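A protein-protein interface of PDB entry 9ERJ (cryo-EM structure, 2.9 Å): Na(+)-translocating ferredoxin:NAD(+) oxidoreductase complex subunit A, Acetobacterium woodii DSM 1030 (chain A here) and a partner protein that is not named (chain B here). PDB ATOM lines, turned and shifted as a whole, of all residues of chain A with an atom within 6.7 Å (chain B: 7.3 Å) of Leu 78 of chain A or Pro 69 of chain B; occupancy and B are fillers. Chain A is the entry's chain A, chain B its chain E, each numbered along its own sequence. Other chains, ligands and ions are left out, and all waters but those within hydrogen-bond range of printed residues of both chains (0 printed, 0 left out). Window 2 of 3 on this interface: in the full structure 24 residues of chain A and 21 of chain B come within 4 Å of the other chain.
Printed residues of chain B within 4 Å of Ile 74 of chain A: Val 73 (3.9 Å) and Ala 76 (3.97 Å).
Ile 79 of chain A touches none of the printed residues of chain B.
Printed residues of chain B within 4 Å of Gln 85 of chain A: Asn 65 and Pro 69.
Printed residues of chain A within 4 Å of Asn 65 of chain B: Gln 85.
Phe 71 of chain B touches none of the printed residues of chain A.
Of the printed residues of chain A, Val 73 of chain B touches Ile 74 (3.9 Å).
Of the printed residues of chain A, Ala 76 of chain B touches Ile 74 (3.97 Å).
The nearest residue of chain B that does not touch Leu 78 of chain A is Val 73 of chain B (4.4 Å).
The nearest residue of chain A that does not touch Pro 69 of chain B is Ala 81 of chain A (4.8 Å).
Among the printed residues, pairs that only touch across the chains: Gln 85 of chain A with Pro 69 of chain B (3.7 Å), Leu 78 of chain A with Pro 69 of chain B (3.8 Å), Gln 85 of chain A with Asn 65 of chain B (3.9 Å), Ile 74 of chain A with Val 73 of chain B (3.9 Å) and Ile 74 of chain A with Ala 76 of chain B (3.97 Å).
Of the 12 printed residues of chain A, 3 touch a printed residue of chain B.
Printed residues of chain B that touch a printed residue of chain A: Asn 65, Pro 69, Val 73 and Ala 76.
Hydrophobic or aromatic side chains of chain B within 4 Å of the printed part of chain A: Pro 69, Val 73 and Ala 76.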
ATOM      1  N   THR A  73     -10.660  10.350 -10.997  1.00  0.00           N
ATOM      2  CA  THR A  73     -12.056  10.586 -10.638  1.00  0.00           C
ATOM      3  C   THR A  73     -12.414  12.064 -10.704  1.00  0.00           C
ATOM      4  O   THR A  73     -13.478  12.428 -11.220  1.00  0.00           O
ATOM      5  CB  THR A  73     -12.338  10.033  -9.241  1.00  0.00           C
ATOM      6  OG1 THR A  73     -11.821   8.701  -9.139  1.00  0.00           O
ATOM      7  CG2 THR A  73     -13.832  10.009  -8.969  1.00  0.00           C
ATOM      8  N   ILE A  74     -11.537  12.933 -10.196  1.00  0.00           N
ATOM      9  CA  ILE A  74     -11.850  14.358 -10.144  1.00  0.00           C
ATOM     10  C   ILE A  74     -11.910  14.955 -11.549  1.00  0.00           C
ATOM     11  O   ILE A  74     -12.830  15.717 -11.871  1.00  0.00           O
ATOM     12  CB  ILE A  74     -10.850  15.091  -9.225  1.00  0.00           C
ATOM     13  CG1 ILE A  74     -11.210  16.572  -9.094  1.00  0.00           C
ATOM     14  CG2 ILE A  74      -9.400  14.878  -9.662  1.00  0.00           C
ATOM     15  CD1 ILE A  74     -10.480  17.273  -7.971  1.00  0.00           C
ATOM     16  N   ALA A  75     -10.964  14.587 -12.419  1.00  0.00           N
ATOM     17  CA  ALA A  75     -10.987  15.082 -13.793  1.00  0.00           C
ATOM     18  C   ALA A  75     -12.193  14.547 -14.555  1.00  0.00           C
ATOM     19  O   ALA A  75     -12.849  15.293 -15.298  1.00  0.00           O
ATOM     20  CB  ALA A  75      -9.690  14.706 -14.506  1.00  0.00           C
ATOM     21  N   PHE A  76     -12.504  13.258 -14.377  1.00  0.00           N
ATOM     22  CA  PHE A  76     -13.643  12.671 -15.075  1.00  0.00           C
ATOM     23  C   PHE A  76     -14.951  13.331 -14.651  1.00  0.00           C
ATOM     24  O   PHE A  76     -15.788  13.672 -15.499  1.00  0.00           O
ATOM     25  CB  PHE A  76     -13.698  11.162 -14.824  1.00  0.00           C
ATOM     26  CG  PHE A  76     -12.698  10.360 -15.625  1.00  0.00           C
ATOM     27  CD1 PHE A  76     -11.629  10.969 -16.263  1.00  0.00           C
ATOM     28  CD2 PHE A  76     -12.834   8.986 -15.735  1.00  0.00           C
ATOM     29  CE1 PHE A  76     -10.718  10.226 -16.990  1.00  0.00           C
ATOM     30  CE2 PHE A  76     -11.928   8.239 -16.463  1.00  0.00           C
ATOM     31  CZ  PHE A  76     -10.870   8.860 -17.090  1.00  0.00           C
ATOM     32  N   ILE A  77     -15.136  13.543 -13.345  1.00  0.00           N
ATOM     33  CA  ILE A  77     -16.378  14.149 -12.878  1.00  0.00           C
ATOM     34  C   ILE A  77     -16.441  15.625 -13.258  1.00  0.00           C
ATOM     35  O   ILE A  77     -17.530  16.150 -13.516  1.00  0.00           O
ATOM     36  CB  ILE A  77     -16.566  13.919 -11.364  1.00  0.00           C
ATOM     37  CG1 ILE A  77     -18.031  14.127 -10.972  1.00  0.00           C
ATOM     38  CG2 ILE A  77     -15.658  14.812 -10.532  1.00  0.00           C
ATOM     39  CD1 ILE A  77     -18.998  13.248 -11.731  1.00  0.00           C
ATOM     40  N   LEU A  78     -15.296  16.313 -13.339  1.00  0.00           N
ATOM     41  CA  LEU A  78     -15.298  17.695 -13.810  1.00  0.00           C
ATOM     42  C   LEU A  78     -15.758  17.779 -15.261  1.00  0.00           C
ATOM     43  O   LEU A  78     -16.594  18.623 -15.614  1.00  0.00           O
ATOM     44  CB  LEU A  78     -13.905  18.304 -13.650  1.00  0.00           C
ATOM     45  CG  LEU A  78     -13.770  19.826 -13.744  1.00  0.00           C
ATOM     46  CD1 LEU A  78     -14.974  20.530 -13.138  1.00  0.00           C
ATOM     47  CD2 LEU A  78     -12.485  20.291 -13.077  1.00  0.00           C
ATOM     48  N   ILE A  79     -15.235  16.892 -16.114  1.00  0.00           N
ATOM     49  CA  ILE A  79     -15.637  16.882 -17.520  1.00  0.00           C
ATOM     50  C   ILE A  79     -17.121  16.551 -17.655  1.00  0.00           C
ATOM     51  O   ILE A  79     -17.853  17.200 -18.417  1.00  0.00           O
ATOM     52  CB  ILE A  79     -14.755  15.903 -18.319  1.00  0.00           C
ATOM     53  CG1 ILE A  79     -13.382  16.521 -18.588  1.00  0.00           C
ATOM     54  CG2 ILE A  79     -15.422  15.504 -19.627  1.00  0.00           C
ATOM     55  CD1 ILE A  79     -12.248  15.523 -18.557  1.00  0.00           C
ATOM     56  N   ILE A  80     -17.591  15.549 -16.905  1.00  0.00           N
ATOM     57  CA  ILE A  80     -18.993  15.145 -16.997  1.00  0.00           C
ATOM     58  C   ILE A  80     -19.914  16.266 -16.523  1.00  0.00           C
ATOM     59  O   ILE A  80     -20.949  16.540 -17.145  1.00  0.00           O
ATOM     60  CB  ILE A  80     -19.222  13.837 -16.215  1.00  0.00           C
ATOM     61  CG1 ILE A  80     -18.735  12.642 -17.036  1.00  0.00           C
ATOM     62  CG2 ILE A  80     -20.689  13.657 -15.858  1.00  0.00           C
ATOM     63  CD1 ILE A  80     -18.157  11.521 -16.208  1.00  0.00           C
ATOM     64  N   ALA A  81     -19.552  16.943 -15.427  1.00  0.00           N
ATOM     65  CA  ALA A  81     -20.366  18.049 -14.933  1.00  0.00           C
ATOM     66  C   ALA A  81     -20.398  19.204 -15.926  1.00  0.00           C
ATOM     67  O   ALA A  81     -21.453  19.817 -16.141  1.00  0.00           O
ATOM     68  CB  ALA A  81     -19.841  18.521 -13.579  1.00  0.00           C
ATOM     69  N   ALA A  82     -19.254  19.516 -16.545  1.00  0.00           N
ATOM     70  CA  ALA A  82     -19.226  20.584 -17.539  1.00  0.00           C
ATOM     71  C   ALA A  82     -20.056  20.236 -18.769  1.00  0.00           C
ATOM     72  O   ALA A  82     -20.614  21.133 -19.412  1.00  0.00           O
ATOM     73  CB  ALA A  82     -17.784  20.894 -17.939  1.00  0.00           C
ATOM     74  N   LEU A  83     -20.147  18.949 -19.118  1.00  0.00           N
ATOM     75  CA  LEU A  83     -21.007  18.557 -20.234  1.00  0.00           C
ATOM     76  C   LEU A  83     -22.485  18.642 -19.859  1.00  0.00           C
ATOM     77  O   LEU A  83     -23.308  19.132 -20.647  1.00  0.00           O
ATOM     78  CB  LEU A  83     -20.657  17.143 -20.696  1.00  0.00           C
ATOM     79  CG  LEU A  83     -19.495  17.022 -21.682  1.00  0.00           C
ATOM     80  CD1 LEU A  83     -18.954  15.602 -21.698  1.00  0.00           C
ATOM     81  CD2 LEU A  83     -19.922  17.458 -23.068  1.00  0.00           C
ATOM     82  N   GLN A  85     -23.866  20.517 -17.669  1.00  0.00           N
ATOM     83  CA  GLN A  85     -24.285  21.914 -17.571  1.00  0.00           C
ATOM     84  C   GLN A  85     -24.722  22.460 -18.928  1.00  0.00           C
ATOM     85  O   GLN A  85     -25.760  23.126 -19.035  1.00  0.00           O
ATOM     86  CB  GLN A  85     -23.155  22.762 -16.991  1.00  0.00           C
ATOM     87  CG  GLN A  85     -23.590  24.149 -16.560  1.00  0.00           C
ATOM     88  CD  GLN A  85     -23.675  24.287 -15.057  1.00  0.00           C
ATOM     89  OE1 GLN A  85     -22.846  23.749 -14.325  1.00  0.00           O
ATOM     90  NE2 GLN A  85     -24.684  25.009 -14.584  1.00  0.00           N
ATOM     91  N   ASN B  65     -23.291  30.221 -11.509  1.00  0.00           N
ATOM     92  CA  ASN B  65     -23.033  29.669 -12.832  1.00  0.00           C
ATOM     93  C   ASN B  65     -22.007  28.545 -12.827  1.00  0.00           C
ATOM     94  O   ASN B  65     -22.005  27.721 -13.746  1.00  0.00           O
ATOM     95  CB  ASN B  65     -22.558  30.775 -13.782  1.00  0.00           C
ATOM     96  CG  ASN B  65     -23.666  31.743 -14.151  1.00  0.00           C
ATOM     97  OD1 ASN B  65     -24.544  31.425 -14.953  1.00  0.00           O
ATOM     98  ND2 ASN B  65     -23.630  32.935 -13.566  1.00  0.00           N
ATOM     99  N   ILE B  66     -21.139  28.493 -11.817  1.00  0.00           N
ATOM    100  CA  ILE B  66     -20.094  27.479 -11.727  1.00  0.00           C
ATOM    101  C   ILE B  66     -20.239  26.715 -10.418  1.00  0.00           C
ATOM    102  O   ILE B  66     -19.242  26.324  -9.801  1.00  0.00           O
ATOM    103  CB  ILE B  66     -18.696  28.110 -11.849  1.00  0.00           C
ATOM    104  CG1 ILE B  66     -18.581  29.336 -10.943  1.00  0.00           C
ATOM    105  CG2 ILE B  66     -18.405  28.482 -13.294  1.00  0.00           C
ATOM    106  CD1 ILE B  66     -17.168  29.645 -10.510  1.00  0.00           C
ATOM    107  N   ARG B  67     -21.481  26.507  -9.981  1.00  0.00           N
ATOM    108  CA  ARG B  67     -21.738  25.921  -8.669  1.00  0.00           C
ATOM    109  C   ARG B  67     -21.416  24.428  -8.636  1.00  0.00           C
ATOM    110  O   ARG B  67     -20.681  23.960  -7.759  1.00  0.00           O
ATOM    111  CB  ARG B  67     -23.197  26.168  -8.275  1.00  0.00           C
ATOM    112  CG  ARG B  67     -23.374  26.790  -6.902  1.00  0.00           C
ATOM    113  CD  ARG B  67     -24.707  27.511  -6.801  1.00  0.00           C
ATOM    114  NE  ARG B  67     -25.786  26.621  -6.392  1.00  0.00           N
ATOM    115  CZ  ARG B  67     -26.919  27.027  -5.832  1.00  0.00           C
ATOM    116  NH1 ARG B  67     -27.158  28.308  -5.609  1.00  0.00           N
ATOM    117  NH2 ARG B  67     -27.833  26.124  -5.490  1.00  0.00           N
ATOM    118  N   ILE B  68     -21.980  23.661  -9.575  1.00  0.00           N
ATOM    119  CA  ILE B  68     -21.779  22.206  -9.566  1.00  0.00           C
ATOM    120  C   ILE B  68     -20.326  21.816  -9.816  1.00  0.00           C
ATOM    121  O   ILE B  68     -19.831  20.902  -9.130  1.00  0.00           O
ATOM    122  CB  ILE B  68     -22.773  21.528 -10.520  1.00  0.00           C
ATOM    123  CG1 ILE B  68     -24.203  21.700 -10.004  1.00  0.00           C
ATOM    124  CG2 ILE B  68     -22.450  20.052 -10.697  1.00  0.00           C
ATOM    125  CD1 ILE B  68     -25.244  20.987 -10.839  1.00  0.00           C
ATOM    126  N   PRO B  69     -19.591  22.412 -10.775  1.00  0.00           N
ATOM    127  CA  PRO B  69     -18.146  22.120 -10.845  1.00  0.00           C
ATOM    128  C   PRO B  69     -17.390  22.458  -9.572  1.00  0.00           C
ATOM    129  O   PRO B  69     -16.421  21.765  -9.239  1.00  0.00           O
ATOM    130  CB  PRO B  69     -17.652  22.977 -12.021  1.00  0.00           C
ATOM    131  CG  PRO B  69     -18.838  23.485 -12.712  1.00  0.00           C
ATOM    132  CD  PRO B  69     -20.072  23.050 -12.016  1.00  0.00           C
ATOM    133  N   ALA B  70     -17.794  23.504  -8.851  1.00  0.00           N
ATOM    134  CA  ALA B  70     -17.126  23.834  -7.597  1.00  0.00           C
ATOM    135  C   ALA B  70     -17.447  22.819  -6.507  1.00  0.00           C
ATOM    136  O   ALA B  70     -16.606  22.547  -5.643  1.00  0.00           O
ATOM    137  CB  ALA B  70     -17.516  25.241  -7.147  1.00  0.00           C
ATOM    138  N   PHE B  71     -18.658  22.259  -6.527  1.00  0.00           N
ATOM    139  CA  PHE B  71     -19.038  21.276  -5.516  1.00  0.00           C
ATOM    140  C   PHE B  71     -18.342  19.939  -5.746  1.00  0.00           C
ATOM    141  O   PHE B  71     -17.838  19.315  -4.796  1.00  0.00           O
ATOM    142  CB  PHE B  71     -20.556  21.086  -5.519  1.00  0.00           C
ATOM    143  CG  PHE B  71     -21.327  22.267  -4.990  1.00  0.00           C
ATOM    144  CD1 PHE B  71     -20.686  23.301  -4.327  1.00  0.00           C
ATOM    145  CD2 PHE B  71     -22.699  22.342  -5.162  1.00  0.00           C
ATOM    146  CE1 PHE B  71     -21.399  24.382  -3.846  1.00  0.00           C
ATOM    147  CE2 PHE B  71     -23.416  23.419  -4.682  1.00  0.00           C
ATOM    148  CZ  PHE B  71     -22.765  24.440  -4.023  1.00  0.00           C
ATOM    149  N   VAL B  72     -18.309  19.481  -7.003  1.00  0.00           N
ATOM    150  CA  VAL B  72     -17.812  18.136  -7.278  1.00  0.00           C
ATOM    151  C   VAL B  72     -16.315  18.038  -7.016  1.00  0.00           C
ATOM    152  O   VAL B  72     -15.815  16.963  -6.678  1.00  0.00           O
ATOM    153  CB  VAL B  72     -18.161  17.695  -8.712  1.00  0.00           C
ATOM    154  CG1 VAL B  72     -19.666  17.535  -8.870  1.00  0.00           C
ATOM    155  CG2 VAL B  72     -17.592  18.659  -9.738  1.00  0.00           C
ATOM    156  N   VAL B  73     -15.579  19.145  -7.146  1.00  0.00           N
ATOM    157  CA  VAL B  73     -14.143  19.125  -6.868  1.00  0.00           C
ATOM    158  C   VAL B  73     -13.889  18.822  -5.395  1.00  0.00           C
ATOM    159  O   VAL B  73     -13.067  17.963  -5.051  1.00  0.00           O
ATOM    160  CB  VAL B  73     -13.498  20.458  -7.293  1.00  0.00           C
ATOM    161  CG1 VAL B  73     -12.121  20.610  -6.673  1.00  0.00           C
ATOM    162  CG2 VAL B  73     -13.409  20.540  -8.806  1.00  0.00           C
ATOM    163  N   VAL B  74     -14.611  19.508  -4.505  1.00  0.00           N
ATOM    164  CA  VAL B  74     -14.463  19.276  -3.070  1.00  0.00           C
ATOM    165  C   VAL B  74     -14.891  17.860  -2.707  1.00  0.00           C
ATOM    166  O   VAL B  74     -14.205  17.158  -1.942  1.00  0.00           O
ATOM    167  CB  VAL B  74     -15.264  20.327  -2.280  1.00  0.00           C
ATOM    168  CG1 VAL B  74     -14.940  20.243  -0.801  1.00  0.00           C
ATOM    169  CG2 VAL B  74     -14.983  21.721  -2.815  1.00  0.00           C
ATOM    170  N   ALA B  76     -14.992  15.164  -4.611  1.00  0.00           N
ATOM    171  CA  ALA B  76     -14.034  14.199  -5.136  1.00  0.00           C
ATOM    172  C   ALA B  76     -12.724  14.216  -4.362  1.00  0.00           C
ATOM    173  O   ALA B  76     -12.105  13.163  -4.190  1.00  0.00           O
ATOM    174  CB  ALA B  76     -13.778  14.466  -6.617  1.00  0.00           C
